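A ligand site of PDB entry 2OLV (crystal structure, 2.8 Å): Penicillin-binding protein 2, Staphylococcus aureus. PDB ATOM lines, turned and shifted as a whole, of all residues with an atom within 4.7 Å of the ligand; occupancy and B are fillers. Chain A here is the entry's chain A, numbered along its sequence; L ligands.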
ATOM      1  N   GLU A  56      35.450  -0.892  24.766  1.00  0.00           N
ATOM      2  CA  GLU A  56      34.087  -1.292  24.357  1.00  0.00           C
ATOM      3  C   GLU A  56      33.120  -1.524  25.513  1.00  0.00           C
ATOM      4  O   GLU A  56      32.011  -0.993  25.495  1.00  0.00           O
ATOM      5  CB  GLU A  56      34.112  -2.552  23.499  1.00  0.00           C
ATOM      6  CG  GLU A  56      34.747  -2.393  22.120  1.00  0.00           C
ATOM      7  CD  GLU A  56      34.134  -1.255  21.290  1.00  0.00           C
ATOM      8  OE1 GLU A  56      33.308  -1.560  20.408  1.00  0.00           O
ATOM      9  OE2 GLU A  56      34.465  -0.075  21.508  1.00  0.00           O
ATOM     10  N   GLY A  87      23.861   5.774  20.687  1.00  0.00           N
ATOM     11  CA  GLY A  87      24.567   5.969  21.962  1.00  0.00           C
ATOM     12  C   GLY A  87      25.751   5.031  22.152  1.00  0.00           C
ATOM     13  O   GLY A  87      26.827   5.247  21.584  1.00  0.00           O
ATOM     14  N   ALA A  88      25.550   3.978  22.968  1.00  0.00           N
ATOM     15  CA  ALA A  88      26.588   2.962  23.240  1.00  0.00           C
ATOM     16  C   ALA A  88      25.953   1.614  23.656  1.00  0.00           C
ATOM     17  O   ALA A  88      24.785   1.537  24.056  1.00  0.00           O
ATOM     18  CB  ALA A  88      27.563   3.469  24.316  1.00  0.00           C
ATOM     19  N   GLN A  93      25.459  -7.805  23.852  1.00  0.00           N
ATOM     20  CA  GLN A  93      24.468  -7.390  22.863  1.00  0.00           C
ATOM     21  C   GLN A  93      25.181  -7.083  21.541  1.00  0.00           C
ATOM     22  O   GLN A  93      24.689  -7.422  20.461  1.00  0.00           O
ATOM     23  CB  GLN A  93      23.587  -6.233  23.392  1.00  0.00           C
ATOM     24  CG  GLN A  93      23.988  -4.802  23.008  1.00  0.00           C
ATOM     25  CD  GLN A  93      23.063  -3.734  23.636  1.00  0.00           C
ATOM     26  OE1 GLN A  93      22.847  -3.726  24.843  1.00  0.00           O
ATOM     27  NE2 GLN A  93      22.543  -2.830  22.805  1.00  0.00           N
ATOM     28  N   GLN A  94      26.357  -6.480  21.643  1.00  0.00           N
ATOM     29  CA  GLN A  94      27.179  -6.190  20.469  1.00  0.00           C
ATOM     30  C   GLN A  94      27.314  -7.473  19.642  1.00  0.00           C
ATOM     31  O   GLN A  94      27.225  -7.442  18.412  1.00  0.00           O
ATOM     32  CB  GLN A  94      28.556  -5.644  20.895  1.00  0.00           C
ATOM     33  CG  GLN A  94      29.216  -4.654  19.908  1.00  0.00           C
ATOM     34  CD  GLN A  94      30.480  -3.974  20.466  1.00  0.00           C
ATOM     35  OE1 GLN A  94      31.513  -3.901  19.795  1.00  0.00           O
ATOM     36  NE2 GLN A  94      30.395  -3.463  21.692  1.00  0.00           N
ATOM     37  N   LYS A  97      23.823  -8.598  17.881  1.00  0.00           N
ATOM     38  CA  LYS A  97      23.729  -7.870  16.616  1.00  0.00           C
ATOM     39  C   LYS A  97      24.455  -8.603  15.489  1.00  0.00           C
ATOM     40  O   LYS A  97      23.987  -8.628  14.351  1.00  0.00           O
ATOM     41  CB  LYS A  97      24.327  -6.463  16.767  1.00  0.00           C
ATOM     42  CG  LYS A  97      24.601  -5.710  15.460  1.00  0.00           C
ATOM     43  CD  LYS A  97      25.006  -4.257  15.708  1.00  0.00           C
ATOM     44  CE  LYS A  97      26.377  -4.153  16.379  1.00  0.00           C
ATOM     45  NZ  LYS A  97      26.950  -2.775  16.325  1.00  0.00           N
ATOM     46  N   ASP A  98      25.611  -9.166  15.806  1.00  0.00           N
ATOM     47  CA  ASP A  98      26.419  -9.882  14.829  1.00  0.00           C
ATOM     48  C   ASP A  98      26.033 -11.365  14.682  1.00  0.00           C
ATOM     49  O   ASP A  98      26.635 -12.087  13.881  1.00  0.00           O
ATOM     50  CB  ASP A  98      27.904  -9.674  15.130  1.00  0.00           C
ATOM     51  CG  ASP A  98      28.372  -8.259  14.808  1.00  0.00           C
ATOM     52  OD1 ASP A  98      28.482  -7.937  13.609  1.00  0.00           O
ATOM     53  OD2 ASP A  98      28.647  -7.473  15.738  1.00  0.00           O
ATOM     54  N   GLN A 103      19.951  -5.086   8.665  1.00  0.00           N
ATOM     55  CA  GLN A 103      20.662  -3.812   8.445  1.00  0.00           C
ATOM     56  C   GLN A 103      19.789  -2.568   8.761  1.00  0.00           C
ATOM     57  O   GLN A 103      20.317  -1.456   8.844  1.00  0.00           O
ATOM     58  CB  GLN A 103      21.248  -3.753   7.019  1.00  0.00           C
ATOM     59  CG  GLN A 103      22.795  -3.773   6.944  1.00  0.00           C
ATOM     60  CD  GLN A 103      23.432  -5.073   7.437  1.00  0.00           C
ATOM     61  OE1 GLN A 103      22.763  -6.100   7.604  1.00  0.00           O
ATOM     62  NE2 GLN A 103      24.742  -5.034   7.657  1.00  0.00           N
ATOM     63  N   LYS A 105      17.649  -0.601  11.674  1.00  0.00           N
ATOM     64  CA  LYS A 105      17.839  -0.496  13.122  1.00  0.00           C
ATOM     65  C   LYS A 105      16.658   0.229  13.784  1.00  0.00           C
ATOM     66  O   LYS A 105      15.652  -0.409  14.100  1.00  0.00           O
ATOM     67  CB  LYS A 105      19.194   0.150  13.439  1.00  0.00           C
ATOM     68  CG  LYS A 105      19.733   1.094  12.375  1.00  0.00           C
ATOM     69  CD  LYS A 105      21.070   1.666  12.762  1.00  0.00           C
ATOM     70  CE  LYS A 105      21.709   2.372  11.592  1.00  0.00           C
ATOM     71  NZ  LYS A 105      23.049   2.924  11.926  1.00  0.00           N
ATOM     72  N   ARG A 109      16.140  -3.346  15.631  1.00  0.00           N
ATOM     73  CA  ARG A 109      17.307  -4.169  15.899  1.00  0.00           C
ATOM     74  C   ARG A 109      17.565  -4.178  17.401  1.00  0.00           C
ATOM     75  O   ARG A 109      17.722  -5.235  18.004  1.00  0.00           O
ATOM     76  CB  ARG A 109      18.525  -3.608  15.164  1.00  0.00           C
ATOM     77  CG  ARG A 109      19.801  -4.400  15.352  1.00  0.00           C
ATOM     78  CD  ARG A 109      20.995  -3.633  14.853  1.00  0.00           C
ATOM     79  NE  ARG A 109      20.907  -3.322  13.429  1.00  0.00           N
ATOM     80  CZ  ARG A 109      21.828  -2.640  12.747  1.00  0.00           C
ATOM     81  NH1 ARG A 109      22.927  -2.203  13.347  1.00  0.00           N
ATOM     82  NH2 ARG A 109      21.645  -2.416  11.457  1.00  0.00           N
ATOM     83  N   LYS A 110      17.571  -2.980  17.994  1.00  0.00           N
ATOM     84  CA  LYS A 110      17.812  -2.780  19.431  1.00  0.00           C
ATOM     85  C   LYS A 110      16.788  -3.490  20.332  1.00  0.00           C
ATOM     86  O   LYS A 110      17.093  -3.866  21.465  1.00  0.00           O
ATOM     87  CB  LYS A 110      17.832  -1.289  19.785  1.00  0.00           C
ATOM     88  CG  LYS A 110      18.858  -0.452  19.014  1.00  0.00           C
ATOM     89  CD  LYS A 110      18.681   1.065  19.239  1.00  0.00           C
ATOM     90  CE  LYS A 110      19.258   1.901  18.091  1.00  0.00           C
ATOM     91  NZ  LYS A 110      19.153   3.365  18.345  1.00  0.00           N
ATOM     92  N   GLU A 113      17.767  -7.314  19.904  1.00  0.00           N
ATOM     93  CA  GLU A 113      19.104  -7.222  20.505  1.00  0.00           C
ATOM     94  C   GLU A 113      19.040  -7.282  22.041  1.00  0.00           C
ATOM     95  O   GLU A 113      19.797  -8.044  22.666  1.00  0.00           O
ATOM     96  CB  GLU A 113      19.758  -5.901  20.047  1.00  0.00           C
ATOM     97  CG  GLU A 113      21.167  -5.620  20.591  1.00  0.00           C
ATOM     98  CD  GLU A 113      21.755  -4.292  20.064  1.00  0.00           C
ATOM     99  OE1 GLU A 113      21.057  -3.257  20.114  1.00  0.00           O
ATOM    100  OE2 GLU A 113      22.921  -4.295  19.618  1.00  0.00           O
ATOM    101  N   TYR A 133      33.050 -12.848  20.387  1.00  0.00           N
ATOM    102  CA  TYR A 133      33.361 -11.480  19.999  1.00  0.00           C
ATOM    103  C   TYR A 133      34.720 -11.481  19.302  1.00  0.00           C
ATOM    104  O   TYR A 133      34.803 -11.171  18.114  1.00  0.00           O
ATOM    105  CB  TYR A 133      33.374 -10.566  21.231  1.00  0.00           C
ATOM    106  CG  TYR A 133      33.538  -9.080  20.958  1.00  0.00           C
ATOM    107  CD1 TYR A 133      34.724  -8.407  21.291  1.00  0.00           C
ATOM    108  CD2 TYR A 133      32.497  -8.333  20.410  1.00  0.00           C
ATOM    109  CE1 TYR A 133      34.874  -7.016  21.051  1.00  0.00           C
ATOM    110  CE2 TYR A 133      32.641  -6.949  20.176  1.00  0.00           C
ATOM    111  CZ  TYR A 133      33.823  -6.296  20.502  1.00  0.00           C
ATOM    112  OH  TYR A 133      33.943  -4.947  20.259  1.00  0.00           O
ATOM    113  N   ILE A 137      34.048 -10.313  14.926  1.00  0.00           N
ATOM    114  CA  ILE A 137      34.015  -8.892  14.522  1.00  0.00           C
ATOM    115  C   ILE A 137      35.003  -8.518  13.388  1.00  0.00           C
ATOM    116  O   ILE A 137      36.013  -9.199  13.176  1.00  0.00           O
ATOM    117  CB  ILE A 137      34.224  -7.954  15.713  1.00  0.00           C
ATOM    118  CG1 ILE A 137      35.611  -8.150  16.339  1.00  0.00           C
ATOM    119  CG2 ILE A 137      33.132  -8.160  16.769  1.00  0.00           C
ATOM    120  CD1 ILE A 137      36.070  -6.917  17.143  1.00  0.00           C
ATOM    121  N   TYR A 138      34.690  -7.422  12.680  1.00  0.00           N
ATOM    122  CA  TYR A 138      35.372  -7.055  11.420  1.00  0.00           C
ATOM    123  C   TYR A 138      36.477  -6.025  11.595  1.00  0.00           C
ATOM    124  O   TYR A 138      36.337  -5.095  12.372  1.00  0.00           O
ATOM    125  CB  TYR A 138      34.366  -6.487  10.419  1.00  0.00           C
ATOM    126  CG  TYR A 138      34.949  -6.271   9.040  1.00  0.00           C
ATOM    127  CD1 TYR A 138      34.915  -5.032   8.414  1.00  0.00           C
ATOM    128  CD2 TYR A 138      35.558  -7.325   8.370  1.00  0.00           C
ATOM    129  CE1 TYR A 138      35.468  -4.849   7.148  1.00  0.00           C
ATOM    130  CE2 TYR A 138      36.098  -7.153   7.115  1.00  0.00           C
ATOM    131  CZ  TYR A 138      36.058  -5.929   6.506  1.00  0.00           C
ATOM    132  OH  TYR A 138      36.620  -5.803   5.247  1.00  0.00           O
ATOM    133  N   ASP A 141      39.527  -4.736   5.152  1.00  0.00           N
ATOM    134  CA  ASP A 141      40.202  -5.612   4.171  1.00  0.00           C
ATOM    135  C   ASP A 141      39.875  -7.105   4.376  1.00  0.00           C
ATOM    136  O   ASP A 141      40.748  -7.973   4.238  1.00  0.00           O
ATOM    137  CB  ASP A 141      41.718  -5.373   4.173  1.00  0.00           C
ATOM    138  CG  ASP A 141      42.105  -3.988   3.652  1.00  0.00           C
ATOM    139  OD1 ASP A 141      43.021  -3.379   4.249  1.00  0.00           O
ATOM    140  OD2 ASP A 141      41.517  -3.496   2.658  1.00  0.00           O
ATOM    141  N   GLY A 142      38.624  -7.396   4.720  1.00  0.00           N
ATOM    142  CA  GLY A 142      38.167  -8.786   4.841  1.00  0.00           C
ATOM    143  C   GLY A 142      38.577  -9.525   6.114  1.00  0.00           C
ATOM    144  O   GLY A 142      38.217 -10.706   6.284  1.00  0.00           O
ATOM    145  N   PRO A 173      37.551  -2.035  15.239  1.00  0.00           N
ATOM    146  CA  PRO A 173      36.194  -2.521  14.933  1.00  0.00           C
ATOM    147  C   PRO A 173      35.051  -1.529  15.158  1.00  0.00           C
ATOM    148  O   PRO A 173      33.899  -1.902  14.911  1.00  0.00           O
ATOM    149  CB  PRO A 173      36.020  -3.709  15.901  1.00  0.00           C
ATOM    150  CG  PRO A 173      37.389  -4.068  16.340  1.00  0.00           C
ATOM    151  CD  PRO A 173      38.164  -2.797  16.340  1.00  0.00           C
ATOM    152  N   GLN A 174      35.327  -0.314  15.622  1.00  0.00           N
ATOM    153  CA  GLN A 174      34.277   0.685  15.759  1.00  0.00           C
ATOM    154  C   GLN A 174      33.806   1.211  14.402  1.00  0.00           C
ATOM    155  O   GLN A 174      32.598   1.258  14.129  1.00  0.00           O
ATOM    156  CB  GLN A 174      34.762   1.834  16.639  1.00  0.00           C
ATOM    157  CG  GLN A 174      33.768   2.937  16.835  1.00  0.00           C
ATOM    158  CD  GLN A 174      34.300   4.011  17.749  1.00  0.00           C
ATOM    159  OE1 GLN A 174      35.136   4.828  17.361  1.00  0.00           O
ATOM    160  NE2 GLN A 174      33.804   4.021  18.983  1.00  0.00           N
ATOM    161  N   VAL A 175      34.751   1.635  13.561  1.00  0.00           N
ATOM    162  CA  VAL A 175      34.453   2.010  12.180  1.00  0.00           C
ATOM    163  C   VAL A 175      35.630   1.553  11.305  1.00  0.00           C
ATOM    164  O   VAL A 175      36.351   2.374  10.751  1.00  0.00           O
ATOM    165  CB  VAL A 175      34.183   3.529  12.041  1.00  0.00           C
ATOM    166  CG1 VAL A 175      33.186   3.979  13.080  1.00  0.00           C
ATOM    167  CG2 VAL A 175      35.458   4.327  12.162  1.00  0.00           C
ATOM    168  N   PRO A 176      35.812   0.240  11.183  1.00  0.00           N
ATOM    169  CA  PRO A 176      37.014  -0.339  10.600  1.00  0.00           C
ATOM    170  C   PRO A 176      37.511   0.413   9.366  1.00  0.00           C
ATOM    171  O   PRO A 176      38.605   0.984   9.397  1.00  0.00           O
ATOM    172  CB  PRO A 176      36.607  -1.775  10.237  1.00  0.00           C
ATOM    173  CG  PRO A 176      35.268  -1.998  10.860  1.00  0.00           C
ATOM    174  CD  PRO A 176      34.857  -0.785  11.626  1.00  0.00           C
ATOM    175  N   ASN A 177      36.692   0.445   8.317  1.00  0.00           N
ATOM    176  CA  ASN A 177      37.099   1.028   7.048  1.00  0.00           C
ATOM    177  C   ASN A 177      37.604   2.477   7.226  1.00  0.00           C
ATOM    178  O   ASN A 177      38.642   2.853   6.664  1.00  0.00           O
ATOM    179  CB  ASN A 177      35.957   0.919   6.015  1.00  0.00           C
ATOM    180  CG  ASN A 177      35.638  -0.527   5.633  1.00  0.00           C
ATOM    181  OD1 ASN A 177      36.498  -1.402   5.657  1.00  0.00           O
ATOM    182  ND2 ASN A 177      34.383  -0.791   5.267  1.00  0.00           N
ATOM    183  N   GLN A 231      43.095  -6.428  -1.901  1.00  0.00           N
ATOM    184  CA  GLN A 231      41.855  -6.926  -2.470  1.00  0.00           C
ATOM    185  C   GLN A 231      42.099  -8.269  -3.157  1.00  0.00           C
ATOM    186  O   GLN A 231      41.179  -8.856  -3.735  1.00  0.00           O
ATOM    187  CB  GLN A 231      41.296  -5.911  -3.471  1.00  0.00           C
ATOM    188  CG  GLN A 231      41.107  -4.505  -2.895  1.00  0.00           C
ATOM    189  CD  GLN A 231      41.508  -3.406  -3.871  1.00  0.00           C
ATOM    190  OE1 GLN A 231      42.327  -3.614  -4.764  1.00  0.00           O
ATOM    191  NE2 GLN A 231      40.943  -2.205  -3.684  1.00  0.00           N
HETATM  192  O1  LIG L   1      22.757   1.601  16.347  1.00  0.00           O
HETATM  193  C1  LIG L   1      23.367   0.721  17.306  1.00  0.00           C
HETATM  194  C2  LIG L   1      22.286  -0.134  17.977  1.00  0.00           C
HETATM  195  O2  LIG L   1      21.345  -0.581  17.276  1.00  0.00           O
HETATM  196  O3  LIG L   1      22.411  -0.353  19.204  1.00  0.00           O
HETATM  197  C3  LIG L   1      24.425  -0.183  16.631  1.00  0.00           C
HETATM  198  O4  LIG L   1      24.292  -0.198  15.196  1.00  0.00           O
HETATM  199  P1  LIG L   1      25.452   0.465  14.312  1.00  0.00           P
HETATM  200  O5  LIG L   1      25.632  -0.491  13.023  1.00  0.00           O
HETATM  201  O6  LIG L   1      25.129   1.861  13.933  1.00  0.00           O
HETATM  202  O7  LIG L   1      26.778   0.345  15.181  1.00  0.00           O
HETATM  203  C4  LIG L   1      27.808   1.347  15.077  1.00  0.00           C
HETATM  204  O8  LIG L   1      27.521   2.448  15.984  1.00  0.00           O
HETATM  205  C5  LIG L   1      27.500   1.964  17.361  1.00  0.00           C
HETATM  206  C6  LIG L   1      26.744   2.904  18.313  1.00  0.00           C
HETATM  207  O9  LIG L   1      27.270   3.254  19.370  1.00  0.00           O
HETATM  208  N1  LIG L   1      25.522   3.283  17.955  1.00  0.00           N
HETATM  209  C7  LIG L   1      28.953   1.613  17.760  1.00  0.00           C
HETATM  210  O10 LIG L   1      28.977   1.254  19.151  1.00  0.00           O
HETATM  211  C8  LIG L   1      29.893   2.790  17.508  1.00  0.00           C
HETATM  212  C9  LIG L   1      29.351   0.391  16.860  1.00  0.00           C
HETATM  213  O11 LIG L   1      30.697  -0.102  17.064  1.00  0.00           O
HETATM  214  C10 LIG L   1      30.622  -0.990  18.081  1.00  0.00           C
HETATM  215  O12 LIG L   1      30.107  -2.090  17.877  1.00  0.00           O
HETATM  216  N2  LIG L   1      31.093  -0.612  19.268  1.00  0.00           N
HETATM  217  C11 LIG L   1      29.151   0.637  15.352  1.00  0.00           C
HETATM  218  O13 LIG L   1      29.200  -0.645  14.665  1.00  0.00           O
HETATM  219  C12 LIG L   1      30.305  -0.766  13.753  1.00  0.00           C
HETATM  220  C13 LIG L   1      30.578  -2.257  13.593  1.00  0.00           C
HETATM  221  C14 LIG L   1      31.633  -2.469  12.513  1.00  0.00           C
HETATM  222  O14 LIG L   1      32.010  -3.841  12.464  1.00  0.00           O
HETATM  223  N3  LIG L   1      30.995  -2.847  14.876  1.00  0.00           N
HETATM  224  C15 LIG L   1      30.446  -3.960  15.373  1.00  0.00           C
HETATM  225  C16 LIG L   1      31.026  -4.406  16.717  1.00  0.00           C
HETATM  226  O15 LIG L   1      29.565  -4.617  14.823  1.00  0.00           O
HETATM  227  O16 LIG L   1      29.929  -0.253  12.475  1.00  0.00           O
HETATM  228  C17 LIG L   1      30.836  -0.526  11.363  1.00  0.00           C
HETATM  229  C18 LIG L   1      30.192   0.007  10.106  1.00  0.00           C
HETATM  230  O17 LIG L   1      30.307   1.440   9.998  1.00  0.00           O
HETATM  231  C19 LIG L   1      29.199   1.962  10.760  1.00  0.00           C
HETATM  232  O18 LIG L   1      27.943   1.564  10.147  1.00  0.00           O
HETATM  233  C20 LIG L   1      26.846   1.868  11.015  1.00  0.00           C
HETATM  234  C21 LIG L   1      25.559   1.251  10.438  1.00  0.00           C
HETATM  235  O19 LIG L   1      25.351   1.694   9.101  1.00  0.00           O
HETATM  236  C22 LIG L   1      26.767   3.405  11.171  1.00  0.00           C
HETATM  237  O20 LIG L   1      25.685   3.748  12.041  1.00  0.00           O
HETATM  238  C23 LIG L   1      28.079   3.998  11.717  1.00  0.00           C
HETATM  239  O21 LIG L   1      28.038   5.423  11.620  1.00  0.00           O
HETATM  240  C24 LIG L   1      29.301   3.478  10.941  1.00  0.00           C
HETATM  241  O22 LIG L   1      30.491   3.786  11.681  1.00  0.00           O
HETATM  242  C25 LIG L   1      31.080  -2.017  11.151  1.00  0.00           C
HETATM  243  O23 LIG L   1      31.979  -2.286  10.033  1.00  0.00           O
HETATM  244  C26 LIG L   1      31.330  -2.719   8.786  1.00  0.00           C
HETATM  245  C27 LIG L   1      32.238  -2.428   7.565  1.00  0.00           C
HETATM  246  C28 LIG L   1      31.914  -3.263   6.308  1.00  0.00           C
HETATM  247  O24 LIG L   1      33.116  -3.411   5.555  1.00  0.00           O
HETATM  248  N4  LIG L   1      32.132  -0.998   7.215  1.00  0.00           N
HETATM  249  C29 LIG L   1      32.766  -0.029   7.865  1.00  0.00           C
HETATM  250  C30 LIG L   1      32.513   1.381   7.324  1.00  0.00           C
HETATM  251  O25 LIG L   1      33.491  -0.194   8.836  1.00  0.00           O
HETATM  252  O26 LIG L   1      30.960  -4.117   8.854  1.00  0.00           O
HETATM  253  C31 LIG L   1      30.199  -4.425   7.657  1.00  0.00           C
HETATM  254  C32 LIG L   1      29.183  -5.570   7.872  1.00  0.00           C
HETATM  255  C33 LIG L   1      31.254  -4.637   6.577  1.00  0.00           C
HETATM  256  O27 LIG L   1      30.614  -5.232   5.416  1.00  0.00           O
HETATM  257  C34 LIG L   1      31.518  -6.061   4.656  1.00  0.00           C
HETATM  258  O28 LIG L   1      32.454  -5.240   3.966  1.00  0.00           O
HETATM  259  C35 LIG L   1      30.853  -6.871   3.543  1.00  0.00           C
HETATM  260  O29 LIG L   1      29.757  -7.624   4.043  1.00  0.00           O
HETATM  261  C36 LIG L   1      31.888  -7.810   2.953  1.00  0.00           C
HETATM  262  O30 LIG L   1      31.299  -8.601   1.910  1.00  0.00           O
HETATM  263  C37 LIG L   1      33.091  -7.005   2.410  1.00  0.00           C
HETATM  264  O31 LIG L   1      32.709  -6.313   1.215  1.00  0.00           O
HETATM  265  C38 LIG L   1      33.582  -5.994   3.470  1.00  0.00           C
HETATM  266  C39 LIG L   1      34.633  -4.988   2.972  1.00  0.00           C
HETATM  267  O32 LIG L   1      34.625  -3.742   3.505  1.00  0.00           O
HETATM  268  N5  LIG L   1      35.526  -5.358   2.038  1.00  0.00           N
HETATM  269  C40 LIG L   1      36.498  -4.593   1.500  1.00  0.00           C
HETATM  270  C41 LIG L   1      36.827  -3.255   1.764  1.00  0.00           C
HETATM  271  O33 LIG L   1      36.259  -2.516   2.566  1.00  0.00           O
HETATM  272  C42 LIG L   1      38.019  -2.805   0.905  1.00  0.00           C
HETATM  273  C43 LIG L   1      38.376  -4.038   0.074  1.00  0.00           C
HETATM  274  C44 LIG L   1      37.361  -5.094   0.527  1.00  0.00           C
HETATM  275  O34 LIG L   1      37.323  -6.370   0.039  1.00  0.00           O
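OE1 of Glu 56 lies within hydrogen-bond range of N2 of the ligand, at 2.7 Å.
An oxygen (O6) of the ligand lies within salt-bridge range of the side-chain amino group (NZ) of Lys 105, 3.1 Å away.
The backbone NH of Asn 177 sits at hydrogen-bond distance from an oxygen (O25) of the ligand (3.3 Å).
The side-chain amide nitrogen (ND2) of Asn 177 sits at hydrogen-bond distance from an oxygen (O24) of the ligand (2.9 Å).
O12 of the ligand sits close to OE1 of Gln 94 (3.0 Å).
NH1 of Arg 109 is in salt-bridge range of O5 of the ligand (3.2 Å).
A nitrogen (N3) of the ligand sits at hydrogen-bond distance from the backbone carbonyl oxygen (O) of Pro 173 (3.1 Å).
The side-chain hydroxyl of Tyr 138 sits close to an oxygen (O32) of the ligand (3.4 Å).
The side-chain amino group of Lys 97 sits at hydrogen-bond distance from an oxygen (O7) of the ligand (3.3 Å).
The side-chain carboxylate of Glu 56 lies close to the side-chain amide oxygen of Gln 94, at 3.0 Å.
The side-chain hydroxyl of Tyr 133 lies close to the side-chain carboxylate of Glu 56 (3.4 Å).
The side-chain hydroxyl (OH) of Tyr 133 is in hydrogen-bond range of the side-chain amide oxygen (OE1) of Gln 94, at 2.7 Å.
The backbone carbonyl oxygen (O) of Gln 103 is in hydrogen-bond range of the guanidinium group (NH2) of Arg 109, 3.1 Å away.
OH of Tyr 138 is in hydrogen-bond range of N of Asp 141 (3.1 Å).
OH of Tyr 138 is in hydrogen-bond range of N of Gly 142 (2.6 Å).
The side-chain carboxylate (OE1) of Glu 113 is in hydrogen-bond range of the side-chain amide nitrogen (NE2) of Gln 93.
The backbone carbonyl oxygen (O) of Gly 87 sits close to an oxygen (O9) of the ligand, 3.0 Å away.
The side-chain carboxylate of Asp 98 sits close to an oxygen (O15) of the ligand (3.1 Å).
O3 of the ligand sits close to OE1 of Glu 113, at 3.3 Å.
O of Gln 174 lies close to O16 of the ligand (3.5 Å).
The backbone nitrogen of Pro 176 lies close to an oxygen (O25) of the ligand (3.3 Å).
Residues that only touch the ligand: Ala 88, Lys 110, Asp 141 and Val 175.
Hydrophobic or aromatic side chains that line the ligand: Tyr 138, Val 175 and Pro 176.
The nearest printed residue that does not touch the ligand is Gln 231 (4.1 Å).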
